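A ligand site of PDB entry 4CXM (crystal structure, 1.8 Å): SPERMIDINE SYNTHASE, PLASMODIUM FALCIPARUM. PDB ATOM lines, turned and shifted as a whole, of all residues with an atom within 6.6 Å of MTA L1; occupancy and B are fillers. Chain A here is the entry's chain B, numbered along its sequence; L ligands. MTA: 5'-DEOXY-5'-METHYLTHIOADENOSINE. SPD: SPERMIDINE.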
ATOM      1  N   TYR A  33      -9.019  -6.503 -24.884  1.00  0.00           N
ATOM      2  CA  TYR A  33      -8.642  -5.400 -24.045  1.00  0.00           C
ATOM      3  C   TYR A  33      -9.117  -5.455 -22.597  1.00  0.00           C
ATOM      4  O   TYR A  33      -8.498  -4.861 -21.749  1.00  0.00           O
ATOM      5  CB  TYR A  33      -9.163  -4.126 -24.696  1.00  0.00           C
ATOM      6  CG  TYR A  33      -8.501  -3.846 -26.027  1.00  0.00           C
ATOM      7  CD1 TYR A  33      -7.273  -3.202 -26.075  1.00  0.00           C
ATOM      8  CD2 TYR A  33      -9.090  -4.240 -27.213  1.00  0.00           C
ATOM      9  CE1 TYR A  33      -6.641  -2.958 -27.256  1.00  0.00           C
ATOM     10  CE2 TYR A  33      -8.464  -4.040 -28.404  1.00  0.00           C
ATOM     11  CZ  TYR A  33      -7.248  -3.392 -28.408  1.00  0.00           C
ATOM     12  OH  TYR A  33      -6.680  -3.112 -29.607  1.00  0.00           O
ATOM     13  N   GLN A  34     -10.200  -6.171 -22.310  1.00  0.00           N
ATOM     14  CA  GLN A  34     -10.835  -6.060 -20.977  1.00  0.00           C
ATOM     15  C   GLN A  34     -11.809  -7.155 -20.737  1.00  0.00           C
ATOM     16  O   GLN A  34     -12.283  -7.779 -21.657  1.00  0.00           O
ATOM     17  CB  GLN A  34     -11.463  -4.649 -20.817  1.00  0.00           C
ATOM     18  CG  GLN A  34     -12.598  -4.268 -21.678  1.00  0.00           C
ATOM     19  CD  GLN A  34     -12.683  -2.692 -21.874  1.00  0.00           C
ATOM     20  OE1 GLN A  34     -12.467  -1.895 -20.944  1.00  0.00           O
ATOM     21  NE2 GLN A  34     -13.027  -2.282 -23.086  1.00  0.00           N
ATOM     22  N   LEU A  48     -23.817  -2.971 -17.595  1.00  0.00           N
ATOM     23  CA  LEU A  48     -22.545  -3.239 -18.283  1.00  0.00           C
ATOM     24  C   LEU A  48     -21.379  -2.996 -17.354  1.00  0.00           C
ATOM     25  O   LEU A  48     -21.206  -1.897 -16.781  1.00  0.00           O
ATOM     26  CB  LEU A  48     -22.367  -2.356 -19.501  1.00  0.00           C
ATOM     27  CG  LEU A  48     -21.052  -2.425 -20.242  1.00  0.00           C
ATOM     28  CD1 LEU A  48     -20.849  -3.821 -20.871  1.00  0.00           C
ATOM     29  CD2 LEU A  48     -20.949  -1.382 -21.310  1.00  0.00           C
ATOM     30  N   LEU A  50     -17.056  -3.437 -16.994  1.00  0.00           N
ATOM     31  CA  LEU A  50     -15.741  -3.583 -17.665  1.00  0.00           C
ATOM     32  C   LEU A  50     -14.653  -3.615 -16.601  1.00  0.00           C
ATOM     33  O   LEU A  50     -14.493  -2.674 -15.797  1.00  0.00           O
ATOM     34  CB  LEU A  50     -15.365  -2.424 -18.611  1.00  0.00           C
ATOM     35  CG  LEU A  50     -16.390  -2.326 -19.755  1.00  0.00           C
ATOM     36  CD1 LEU A  50     -16.044  -1.190 -20.700  1.00  0.00           C
ATOM     37  CD2 LEU A  50     -16.422  -3.629 -20.568  1.00  0.00           C
ATOM     38  N   GLN A  55     -20.053   0.426 -15.822  1.00  0.00           N
ATOM     39  CA  GLN A  55     -19.992   1.496 -16.798  1.00  0.00           C
ATOM     40  C   GLN A  55     -21.322   2.127 -17.000  1.00  0.00           C
ATOM     41  O   GLN A  55     -21.397   3.313 -17.268  1.00  0.00           O
ATOM     42  CB  GLN A  55     -19.608   0.861 -18.145  1.00  0.00           C
ATOM     43  CG  GLN A  55     -18.262   0.199 -18.156  1.00  0.00           C
ATOM     44  CD  GLN A  55     -17.169   1.104 -17.715  1.00  0.00           C
ATOM     45  OE1 GLN A  55     -16.542   0.910 -16.627  1.00  0.00           O
ATOM     46  NE2 GLN A  55     -16.925   2.106 -18.508  1.00  0.00           N
ATOM     47  N   LEU A  56     -22.367   1.329 -16.967  1.00  0.00           N
ATOM     48  CA  LEU A  56     -23.755   1.804 -17.052  1.00  0.00           C
ATOM     49  C   LEU A  56     -24.778   0.851 -16.544  1.00  0.00           C
ATOM     50  O   LEU A  56     -24.529  -0.307 -16.497  1.00  0.00           O
ATOM     51  CB  LEU A  56     -24.132   2.320 -18.464  1.00  0.00           C
ATOM     52  CG  LEU A  56     -24.064   1.242 -19.525  1.00  0.00           C
ATOM     53  CD1 LEU A  56     -25.332   0.416 -19.516  1.00  0.00           C
ATOM     54  CD2 LEU A  56     -23.901   1.983 -20.881  1.00  0.00           C
ATOM     55  N   TYR A  64     -25.984  10.525 -17.027  1.00  0.00           N
ATOM     56  CA  TYR A  64     -24.656  10.709 -17.503  1.00  0.00           C
ATOM     57  C   TYR A  64     -24.644  11.119 -19.004  1.00  0.00           C
ATOM     58  O   TYR A  64     -24.003  12.097 -19.433  1.00  0.00           O
ATOM     59  CB  TYR A  64     -23.861   9.412 -17.231  1.00  0.00           C
ATOM     60  CG  TYR A  64     -22.470   9.463 -17.812  1.00  0.00           C
ATOM     61  CD1 TYR A  64     -21.463  10.265 -17.205  1.00  0.00           C
ATOM     62  CD2 TYR A  64     -22.142   8.698 -18.910  1.00  0.00           C
ATOM     63  CE1 TYR A  64     -20.171  10.229 -17.697  1.00  0.00           C
ATOM     64  CE2 TYR A  64     -20.862   8.646 -19.432  1.00  0.00           C
ATOM     65  CZ  TYR A  64     -19.884   9.424 -18.825  1.00  0.00           C
ATOM     66  OH  TYR A  64     -18.614   9.435 -19.289  1.00  0.00           O
ATOM     67  N   HIS A  65     -25.340  10.338 -19.791  1.00  0.00           N
ATOM     68  CA  HIS A  65     -25.303  10.580 -21.253  1.00  0.00           C
ATOM     69  C   HIS A  65     -25.903  11.923 -21.621  1.00  0.00           C
ATOM     70  O   HIS A  65     -25.388  12.600 -22.489  1.00  0.00           O
ATOM     71  CB  HIS A  65     -25.889   9.422 -22.043  1.00  0.00           C
ATOM     72  CG  HIS A  65     -25.096   8.173 -21.871  1.00  0.00           C
ATOM     73  ND1 HIS A  65     -25.674   6.990 -21.536  1.00  0.00           N
ATOM     74  CD2 HIS A  65     -23.793   7.928 -22.055  1.00  0.00           C
ATOM     75  CE1 HIS A  65     -24.731   6.055 -21.397  1.00  0.00           C
ATOM     76  NE2 HIS A  65     -23.579   6.605 -21.708  1.00  0.00           N
ATOM     77  N   VAL A  85     -14.960   9.981 -27.858  1.00  0.00           N
ATOM     78  CA  VAL A  85     -13.839   9.159 -27.552  1.00  0.00           C
ATOM     79  C   VAL A  85     -14.372   8.160 -26.543  1.00  0.00           C
ATOM     80  O   VAL A  85     -14.941   8.542 -25.525  1.00  0.00           O
ATOM     81  CB  VAL A  85     -12.740   9.972 -26.928  1.00  0.00           C
ATOM     82  CG1 VAL A  85     -11.716   9.097 -26.218  1.00  0.00           C
ATOM     83  CG2 VAL A  85     -12.047  10.911 -27.951  1.00  0.00           C
ATOM     84  N   GLY A  86     -14.173   6.878 -26.805  1.00  0.00           N
ATOM     85  CA  GLY A  86     -14.699   5.839 -25.969  1.00  0.00           C
ATOM     86  C   GLY A  86     -16.184   5.703 -26.303  1.00  0.00           C
ATOM     87  O   GLY A  86     -16.565   5.736 -27.476  1.00  0.00           O
ATOM     88  N   GLY A  87     -17.036   5.522 -25.278  1.00  0.00           N
ATOM     89  CA  GLY A  87     -18.497   5.532 -25.526  1.00  0.00           C
ATOM     90  C   GLY A  87     -19.050   4.441 -26.424  1.00  0.00           C
ATOM     91  O   GLY A  87     -20.043   4.616 -27.064  1.00  0.00           O
ATOM     92  N   GLY A  88     -18.394   3.267 -26.440  1.00  0.00           N
ATOM     93  CA  GLY A  88     -18.848   2.156 -27.270  1.00  0.00           C
ATOM     94  C   GLY A  88     -20.288   1.735 -27.067  1.00  0.00           C
ATOM     95  O   GLY A  88     -20.904   1.155 -27.978  1.00  0.00           O
ATOM     96  N   ASP A  89     -20.874   1.995 -25.885  1.00  0.00           N
ATOM     97  CA  ASP A  89     -22.258   1.612 -25.639  1.00  0.00           C
ATOM     98  C   ASP A  89     -23.196   2.392 -26.567  1.00  0.00           C
ATOM     99  O   ASP A  89     -24.281   1.980 -26.817  1.00  0.00           O
ATOM    100  CB  ASP A  89     -22.656   1.921 -24.201  1.00  0.00           C
ATOM    101  CG  ASP A  89     -22.198   3.322 -23.796  1.00  0.00           C
ATOM    102  OD1 ASP A  89     -21.033   3.448 -23.409  1.00  0.00           O
ATOM    103  OD2 ASP A  89     -22.991   4.265 -23.907  1.00  0.00           O
ATOM    104  N   CYS A 108     -14.486   6.954 -31.646  1.00  0.00           N
ATOM    105  CA  CYS A 108     -13.256   6.175 -31.654  1.00  0.00           C
ATOM    106  C   CYS A 108     -13.258   5.362 -30.389  1.00  0.00           C
ATOM    107  O   CYS A 108     -13.116   5.977 -29.341  1.00  0.00           O
ATOM    108  CB  CYS A 108     -12.099   7.127 -31.713  1.00  0.00           C
ATOM    109  SG  CYS A 108     -10.495   6.271 -31.765  1.00  0.00           S
ATOM    110  N   GLU A 109     -13.447   4.053 -30.491  1.00  0.00           N
ATOM    111  CA  GLU A 109     -13.707   3.127 -29.438  1.00  0.00           C
ATOM    112  C   GLU A 109     -12.619   2.027 -29.630  1.00  0.00           C
ATOM    113  O   GLU A 109     -12.444   1.568 -30.754  1.00  0.00           O
ATOM    114  CB  GLU A 109     -15.141   2.518 -29.519  1.00  0.00           C
ATOM    115  CG  GLU A 109     -15.274   1.192 -28.729  1.00  0.00           C
ATOM    116  CD  GLU A 109     -14.996   1.335 -27.180  1.00  0.00           C
ATOM    117  OE1 GLU A 109     -15.737   2.128 -26.490  1.00  0.00           O
ATOM    118  OE2 GLU A 109     -14.055   0.643 -26.670  1.00  0.00           O
ATOM    119  N   ILE A 110     -11.856   1.700 -28.609  1.00  0.00           N
ATOM    120  CA  ILE A 110     -10.768   0.747 -28.735  1.00  0.00           C
ATOM    121  C   ILE A 110     -11.252  -0.688 -28.859  1.00  0.00           C
ATOM    122  O   ILE A 110     -10.587  -1.494 -29.480  1.00  0.00           O
ATOM    123  CB  ILE A 110      -9.754   0.884 -27.568  1.00  0.00           C
ATOM    124  CG1 ILE A 110      -8.402   0.267 -27.957  1.00  0.00           C
ATOM    125  CG2 ILE A 110     -10.349   0.408 -26.289  1.00  0.00           C
ATOM    126  CD1 ILE A 110      -7.291   0.626 -27.052  1.00  0.00           C
ATOM    127  N   ASP A 111     -12.418  -0.955 -28.282  1.00  0.00           N
ATOM    128  CA  ASP A 111     -12.905  -2.296 -28.070  1.00  0.00           C
ATOM    129  C   ASP A 111     -14.206  -2.585 -28.762  1.00  0.00           C
ATOM    130  O   ASP A 111     -15.325  -2.365 -28.245  1.00  0.00           O
ATOM    131  CB  ASP A 111     -13.074  -2.589 -26.583  1.00  0.00           C
ATOM    132  CG  ASP A 111     -13.209  -4.118 -26.291  1.00  0.00           C
ATOM    133  OD1 ASP A 111     -13.607  -4.885 -27.182  1.00  0.00           O
ATOM    134  OD2 ASP A 111     -12.979  -4.488 -25.130  1.00  0.00           O
ATOM    135  N   VAL A 114     -17.368  -4.139 -27.137  1.00  0.00           N
ATOM    136  CA  VAL A 114     -18.307  -3.349 -26.318  1.00  0.00           C
ATOM    137  C   VAL A 114     -19.456  -2.861 -27.233  1.00  0.00           C
ATOM    138  O   VAL A 114     -20.588  -2.826 -26.815  1.00  0.00           O
ATOM    139  CB  VAL A 114     -17.572  -2.124 -25.675  1.00  0.00           C
ATOM    140  CG1 VAL A 114     -18.588  -1.187 -24.988  1.00  0.00           C
ATOM    141  CG2 VAL A 114     -16.539  -2.610 -24.676  1.00  0.00           C
ATOM    142  N   ILE A 115     -19.106  -2.422 -28.436  1.00  0.00           N
ATOM    143  CA  ILE A 115     -20.171  -2.019 -29.419  1.00  0.00           C
ATOM    144  C   ILE A 115     -21.114  -3.173 -29.709  1.00  0.00           C
ATOM    145  O   ILE A 115     -22.333  -3.035 -29.667  1.00  0.00           O
ATOM    146  CB  ILE A 115     -19.505  -1.478 -30.699  1.00  0.00           C
ATOM    147  CG1 ILE A 115     -18.614  -0.304 -30.350  1.00  0.00           C
ATOM    148  CG2 ILE A 115     -20.632  -1.036 -31.641  1.00  0.00           C
ATOM    149  CD1 ILE A 115     -17.802   0.295 -31.461  1.00  0.00           C
ATOM    150  N   GLU A 139      -9.946   1.954 -32.545  1.00  0.00           N
ATOM    151  CA  GLU A 139      -8.589   2.420 -32.400  1.00  0.00           C
ATOM    152  C   GLU A 139      -8.431   3.017 -31.012  1.00  0.00           C
ATOM    153  O   GLU A 139      -9.439   3.463 -30.415  1.00  0.00           O
ATOM    154  CB  GLU A 139      -8.398   3.537 -33.458  1.00  0.00           C
ATOM    155  CG  GLU A 139      -6.984   3.949 -33.721  1.00  0.00           C
ATOM    156  CD  GLU A 139      -6.808   4.876 -34.935  1.00  0.00           C
ATOM    157  OE1 GLU A 139      -7.656   4.884 -35.831  1.00  0.00           O
ATOM    158  OE2 GLU A 139      -5.785   5.573 -35.006  1.00  0.00           O
ATOM    159  N   ASP A 140      -7.197   3.068 -30.510  1.00  0.00           N
ATOM    160  CA  ASP A 140      -6.903   3.763 -29.284  1.00  0.00           C
ATOM    161  C   ASP A 140      -7.035   5.239 -29.655  1.00  0.00           C
ATOM    162  O   ASP A 140      -6.382   5.683 -30.522  1.00  0.00           O
ATOM    163  CB  ASP A 140      -5.495   3.455 -28.811  1.00  0.00           C
ATOM    164  CG  ASP A 140      -5.174   4.034 -27.470  1.00  0.00           C
ATOM    165  OD1 ASP A 140      -5.655   5.098 -27.011  1.00  0.00           O
ATOM    166  OD2 ASP A 140      -4.338   3.397 -26.796  1.00  0.00           O
ATOM    167  N   ALA A 141      -7.902   5.955 -28.949  1.00  0.00           N
ATOM    168  CA  ALA A 141      -8.095   7.367 -29.225  1.00  0.00           C
ATOM    169  C   ALA A 141      -6.857   8.185 -29.141  1.00  0.00           C
ATOM    170  O   ALA A 141      -6.723   9.207 -29.783  1.00  0.00           O
ATOM    171  CB  ALA A 141      -9.229   7.919 -28.379  1.00  0.00           C
ATOM    172  N   SER A 142      -5.900   7.778 -28.324  1.00  0.00           N
ATOM    173  CA  SER A 142      -4.657   8.485 -28.206  1.00  0.00           C
ATOM    174  C   SER A 142      -3.885   8.385 -29.511  1.00  0.00           C
ATOM    175  O   SER A 142      -3.186   9.257 -29.874  1.00  0.00           O
ATOM    176  CB  SER A 142      -3.795   7.761 -27.117  1.00  0.00           C
ATOM    177  OG  SER A 142      -2.688   8.556 -26.979  1.00  0.00           O
ATOM    178  N   ASP A 158     -15.765  10.027 -23.280  1.00  0.00           N
ATOM    179  CA  ASP A 158     -16.566   9.113 -22.553  1.00  0.00           C
ATOM    180  C   ASP A 158     -15.725   7.823 -22.287  1.00  0.00           C
ATOM    181  O   ASP A 158     -16.038   6.743 -22.778  1.00  0.00           O
ATOM    182  CB  ASP A 158     -17.862   8.738 -23.239  1.00  0.00           C
ATOM    183  CG  ASP A 158     -18.701   7.789 -22.368  1.00  0.00           C
ATOM    184  OD1 ASP A 158     -18.371   7.602 -21.144  1.00  0.00           O
ATOM    185  OD2 ASP A 158     -19.708   7.230 -22.874  1.00  0.00           O
ATOM    186  N   SER A 159     -14.688   7.965 -21.504  1.00  0.00           N
ATOM    187  CA  SER A 159     -13.751   6.875 -21.274  1.00  0.00           C
ATOM    188  C   SER A 159     -14.187   5.994 -20.084  1.00  0.00           C
ATOM    189  O   SER A 159     -14.958   6.398 -19.199  1.00  0.00           O
ATOM    190  CB  SER A 159     -12.344   7.470 -20.880  1.00  0.00           C
ATOM    191  OG  SER A 159     -12.588   8.373 -19.780  1.00  0.00           O
ATOM    192  N   SER A 160     -13.604   4.796 -20.066  1.00  0.00           N
ATOM    193  CA  SER A 160     -13.562   4.033 -18.847  1.00  0.00           C
ATOM    194  C   SER A 160     -12.475   4.663 -17.964  1.00  0.00           C
ATOM    195  O   SER A 160     -11.875   5.696 -18.314  1.00  0.00           O
ATOM    196  CB  SER A 160     -13.296   2.558 -19.191  1.00  0.00           C
ATOM    197  OG  SER A 160     -12.163   2.478 -20.045  1.00  0.00           O
ATOM    198  N   ASP A 161     -12.258   4.046 -16.813  1.00  0.00           N
ATOM    199  CA  ASP A 161     -11.360   4.575 -15.755  1.00  0.00           C
ATOM    200  C   ASP A 161      -9.864   4.341 -16.047  1.00  0.00           C
ATOM    201  O   ASP A 161      -9.526   3.517 -16.919  1.00  0.00           O
ATOM    202  CB  ASP A 161     -11.748   3.973 -14.442  1.00  0.00           C
ATOM    203  CG  ASP A 161     -13.110   4.476 -13.972  1.00  0.00           C
ATOM    204  OD1 ASP A 161     -13.407   5.699 -14.068  1.00  0.00           O
ATOM    205  OD2 ASP A 161     -13.906   3.629 -13.621  1.00  0.00           O
ATOM    206  N   GLY A 164      -6.733   0.027 -17.148  1.00  0.00           N
ATOM    207  CA  GLY A 164      -7.272  -0.675 -18.342  1.00  0.00           C
ATOM    208  C   GLY A 164      -6.873   0.185 -19.567  1.00  0.00           C
ATOM    209  O   GLY A 164      -5.987   1.010 -19.512  1.00  0.00           O
ATOM    210  N   PRO A 165      -7.570   0.020 -20.698  1.00  0.00           N
ATOM    211  CA  PRO A 165      -7.122   0.695 -21.955  1.00  0.00           C
ATOM    212  C   PRO A 165      -7.255   2.193 -21.936  1.00  0.00           C
ATOM    213  O   PRO A 165      -6.683   2.914 -22.821  1.00  0.00           O
ATOM    214  CB  PRO A 165      -8.005   0.042 -23.020  1.00  0.00           C
ATOM    215  CG  PRO A 165      -9.179  -0.585 -22.271  1.00  0.00           C
ATOM    216  CD  PRO A 165      -8.683  -0.919 -20.895  1.00  0.00           C
ATOM    217  N   ALA A 166      -8.013   2.734 -20.969  1.00  0.00           N
ATOM    218  CA  ALA A 166      -8.168   4.208 -20.943  1.00  0.00           C
ATOM    219  C   ALA A 166      -6.945   4.888 -20.282  1.00  0.00           C
ATOM    220  O   ALA A 166      -6.927   6.114 -20.114  1.00  0.00           O
ATOM    221  CB  ALA A 166      -9.463   4.620 -20.223  1.00  0.00           C
ATOM    222  N   GLU A 167      -5.936   4.110 -19.896  1.00  0.00           N
ATOM    223  CA  GLU A 167      -4.777   4.718 -19.211  1.00  0.00           C
ATOM    224  C   GLU A 167      -4.135   5.876 -20.036  1.00  0.00           C
ATOM    225  O   GLU A 167      -3.690   6.896 -19.468  1.00  0.00           O
ATOM    226  CB  GLU A 167      -3.753   3.641 -18.839  1.00  0.00           C
ATOM    227  CG  GLU A 167      -3.161   2.902 -20.034  1.00  0.00           C
ATOM    228  CD  GLU A 167      -2.445   1.600 -19.629  1.00  0.00           C
ATOM    229  OE1 GLU A 167      -1.888   1.520 -18.519  1.00  0.00           O
ATOM    230  OE2 GLU A 167      -2.457   0.638 -20.434  1.00  0.00           O
ATOM    231  N   THR A 168      -4.206   5.770 -21.349  1.00  0.00           N
ATOM    232  CA  THR A 168      -3.632   6.829 -22.296  1.00  0.00           C
ATOM    233  C   THR A 168      -4.421   8.133 -22.381  1.00  0.00           C
ATOM    234  O   THR A 168      -3.956   9.197 -22.953  1.00  0.00           O
ATOM    235  CB  THR A 168      -3.520   6.224 -23.743  1.00  0.00           C
ATOM    236  OG1 THR A 168      -4.782   5.645 -24.118  1.00  0.00           O
ATOM    237  CG2 THR A 168      -2.540   5.026 -23.777  1.00  0.00           C
ATOM    238  N   LEU A 169      -5.602   8.112 -21.746  1.00  0.00           N
ATOM    239  CA  LEU A 169      -6.522   9.252 -21.858  1.00  0.00           C
ATOM    240  C   LEU A 169      -6.547  10.266 -20.711  1.00  0.00           C
ATOM    241  O   LEU A 169      -7.394  11.196 -20.689  1.00  0.00           O
ATOM    242  CB  LEU A 169      -7.925   8.730 -22.058  1.00  0.00           C
ATOM    243  CG  LEU A 169      -8.031   7.615 -23.124  1.00  0.00           C
ATOM    244  CD1 LEU A 169      -9.519   7.230 -23.270  1.00  0.00           C
ATOM    245  CD2 LEU A 169      -7.438   8.038 -24.477  1.00  0.00           C
HETATM  246  CS  MTA L   1     -18.380   2.010 -22.169  1.00  0.00           C
HETATM  247  S5' MTA L   1     -18.003   3.720 -22.214  1.00  0.00           S
HETATM  248  C5' MTA L   1     -16.241   3.675 -21.971  1.00  0.00           C
HETATM  249  C4' MTA L   1     -15.368   3.111 -23.096  1.00  0.00           C
HETATM  250  O4' MTA L   1     -14.065   3.617 -23.292  1.00  0.00           O
HETATM  251  C2' MTA L   1     -13.794   1.397 -23.480  1.00  0.00           C
HETATM  252  O2' MTA L   1     -13.467   0.258 -24.294  1.00  0.00           O
HETATM  253  C3' MTA L   1     -15.274   1.610 -23.206  1.00  0.00           C
HETATM  254  O3' MTA L   1     -16.112   1.005 -24.170  1.00  0.00           O
HETATM  255  C1' MTA L   1     -13.390   2.709 -24.153  1.00  0.00           C
HETATM  256  N9  MTA L   1     -11.979   2.969 -24.151  1.00  0.00           N
HETATM  257  C8  MTA L   1     -11.108   2.731 -23.126  1.00  0.00           C
HETATM  258  N7  MTA L   1      -9.874   3.111 -23.460  1.00  0.00           N
HETATM  259  C5  MTA L   1      -9.959   3.652 -24.670  1.00  0.00           C
HETATM  260  C6  MTA L   1      -9.007   4.261 -25.561  1.00  0.00           C
HETATM  261  N6  MTA L   1      -7.722   4.372 -25.218  1.00  0.00           N
HETATM  262  N1  MTA L   1      -9.477   4.698 -26.769  1.00  0.00           N
HETATM  263  C2  MTA L   1     -10.764   4.556 -27.112  1.00  0.00           C
HETATM  264  N3  MTA L   1     -11.674   4.043 -26.335  1.00  0.00           N
HETATM  265  C4  MTA L   1     -11.328   3.538 -25.114  1.00  0.00           C
HETATM  266  N1  SPD L   2     -16.531   4.683 -12.909  1.00  0.00           N
HETATM  267  C2  SPD L   2     -16.983   4.440 -14.300  1.00  0.00           C
HETATM  268  C3  SPD L   2     -17.178   5.615 -15.241  1.00  0.00           C
HETATM  269  C4  SPD L   2     -17.340   5.058 -16.682  1.00  0.00           C
HETATM  270  C5  SPD L   2     -17.986   6.100 -17.563  1.00  0.00           C
HETATM  271  N6  SPD L   2     -17.793   5.796 -18.968  1.00  0.00           N
HETATM  272  C7  SPD L   2     -18.583   4.868 -19.761  1.00  0.00           C
HETATM  273  C8  SPD L   2     -20.023   4.465 -19.454  1.00  0.00           C
HETATM  274  C9  SPD L   2     -21.207   5.176 -20.187  1.00  0.00           C
HETATM  275  N10 SPD L   2     -21.052   5.392 -21.617  1.00  0.00           N
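OE2 of Glu 109 is in hydrogen-bond range of O2' of MTA L1 (2.5 Å).
The side-chain carboxylate (OD1) of Asp 140 is in hydrogen-bond range of a nitrogen (N6) of MTA L1, at 2.8 Å.
The side-chain amide nitrogen (NE2) of Gln 34 lies within hydrogen-bond range of an oxygen (O2') of MTA L1 (2.8 Å).
N1 of MTA L1 sits at hydrogen-bond distance from N of Ala 141.
The backbone carbonyl oxygen of Pro 165 lies within hydrogen-bond range of a nitrogen (N6) of MTA L1 (3.0 Å).
N of Ala 166 is in hydrogen-bond range of N7 of MTA L1 (3.1 Å).
O4' of MTA L1 sits close to N of Ser 160 (3.5 Å).
N of Ile 110 sits at hydrogen-bond distance from N3 of MTA L1, 3.3 Å away.
OG1 of Thr 168 lies within hydrogen-bond range of N6 of MTA L1 (3.4 Å).
The backbone NH (N) of Gly 87 sits close to a sulfur (S5') of MTA L1.
The side-chain carboxylate of Asp 158 is in salt-bridge range of a nitrogen (N10) of SPD L2 (2.6 Å).
A nitrogen (N10) of SPD L2 lies within salt-bridge range of the side-chain carboxylate (OD1) of Asp 89 (2.6 Å).
O of Ser 159 sits at hydrogen-bond distance from N6 of SPD L2, 2.9 Å away.
A nitrogen (N10) of SPD L2 is in hydrogen-bond range of a ring nitrogen (NE2) of His 65 (2.8 Å).
The side-chain carboxylate (OD2) of Asp 161 lies within salt-bridge range of a nitrogen (N1) of SPD L2.
A nitrogen (N10) of SPD L2 lies close to a sulfur (S5') of MTA L1.
OE1 of Glu 109 sits at hydrogen-bond distance from N of Gly 88 (2.9 Å).
OD1 of Asp 140 sits at hydrogen-bond distance from OG1 of Thr 168, at 3.1 Å.
N of Ser 142 lies within hydrogen-bond range of OD1 of Asp 140 (3.0 Å).
O of Asp 158 lies within hydrogen-bond range of N of Gly 87.
OH of Tyr 64 sits at hydrogen-bond distance from OD1 of Asp 158, at 2.6 Å.
A ring nitrogen (NE2) of His 65 is in hydrogen-bond range of the side-chain carboxylate (OD2) of Asp 89, at 3.3 Å.
N of Ile 110 lies close to O of Glu 139, at 3.5 Å.
The backbone carbonyl oxygen (O) of Leu 48 sits at hydrogen-bond distance from the backbone NH (N) of Gln 55.
The side-chain carboxylate of Asp 89 lies close to a sulfur (S5') of MTA L1 (3.3 Å).
The backbone carbonyl oxygen (O) of Asp 158 sits close to a sulfur (S5') of MTA L1 (3.6 Å).
Leu 50 touches MTA L1.
NE2 of Gln 55 touches C5' of MTA L1 (3.9 Å).
CA of Gly 86 touches O4' of MTA L1 (3.5 Å).
Gly 88 touches MTA L1 (N to O3', 3.9 Å).
Cys 108 touches MTA L1.
CB of Asp 111 touches O2' of MTA L1, 3.7 Å away.
CG1 of Val 114 touches O3' of MTA L1, 3.4 Å away.
Glu 139 touches MTA L1 (O to C2, 3.7 Å).
Ser 159 touches MTA L1 (C to C5', 3.6 Å).
CD2 of Leu 169 touches N6 of MTA L1 (3.8 Å).
Of the 33 residues printed, 22 come within 4 Å of MTA L1.
The nearest printed residue that does not touch MTA L1 is Leu 48 (4.3 Å).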
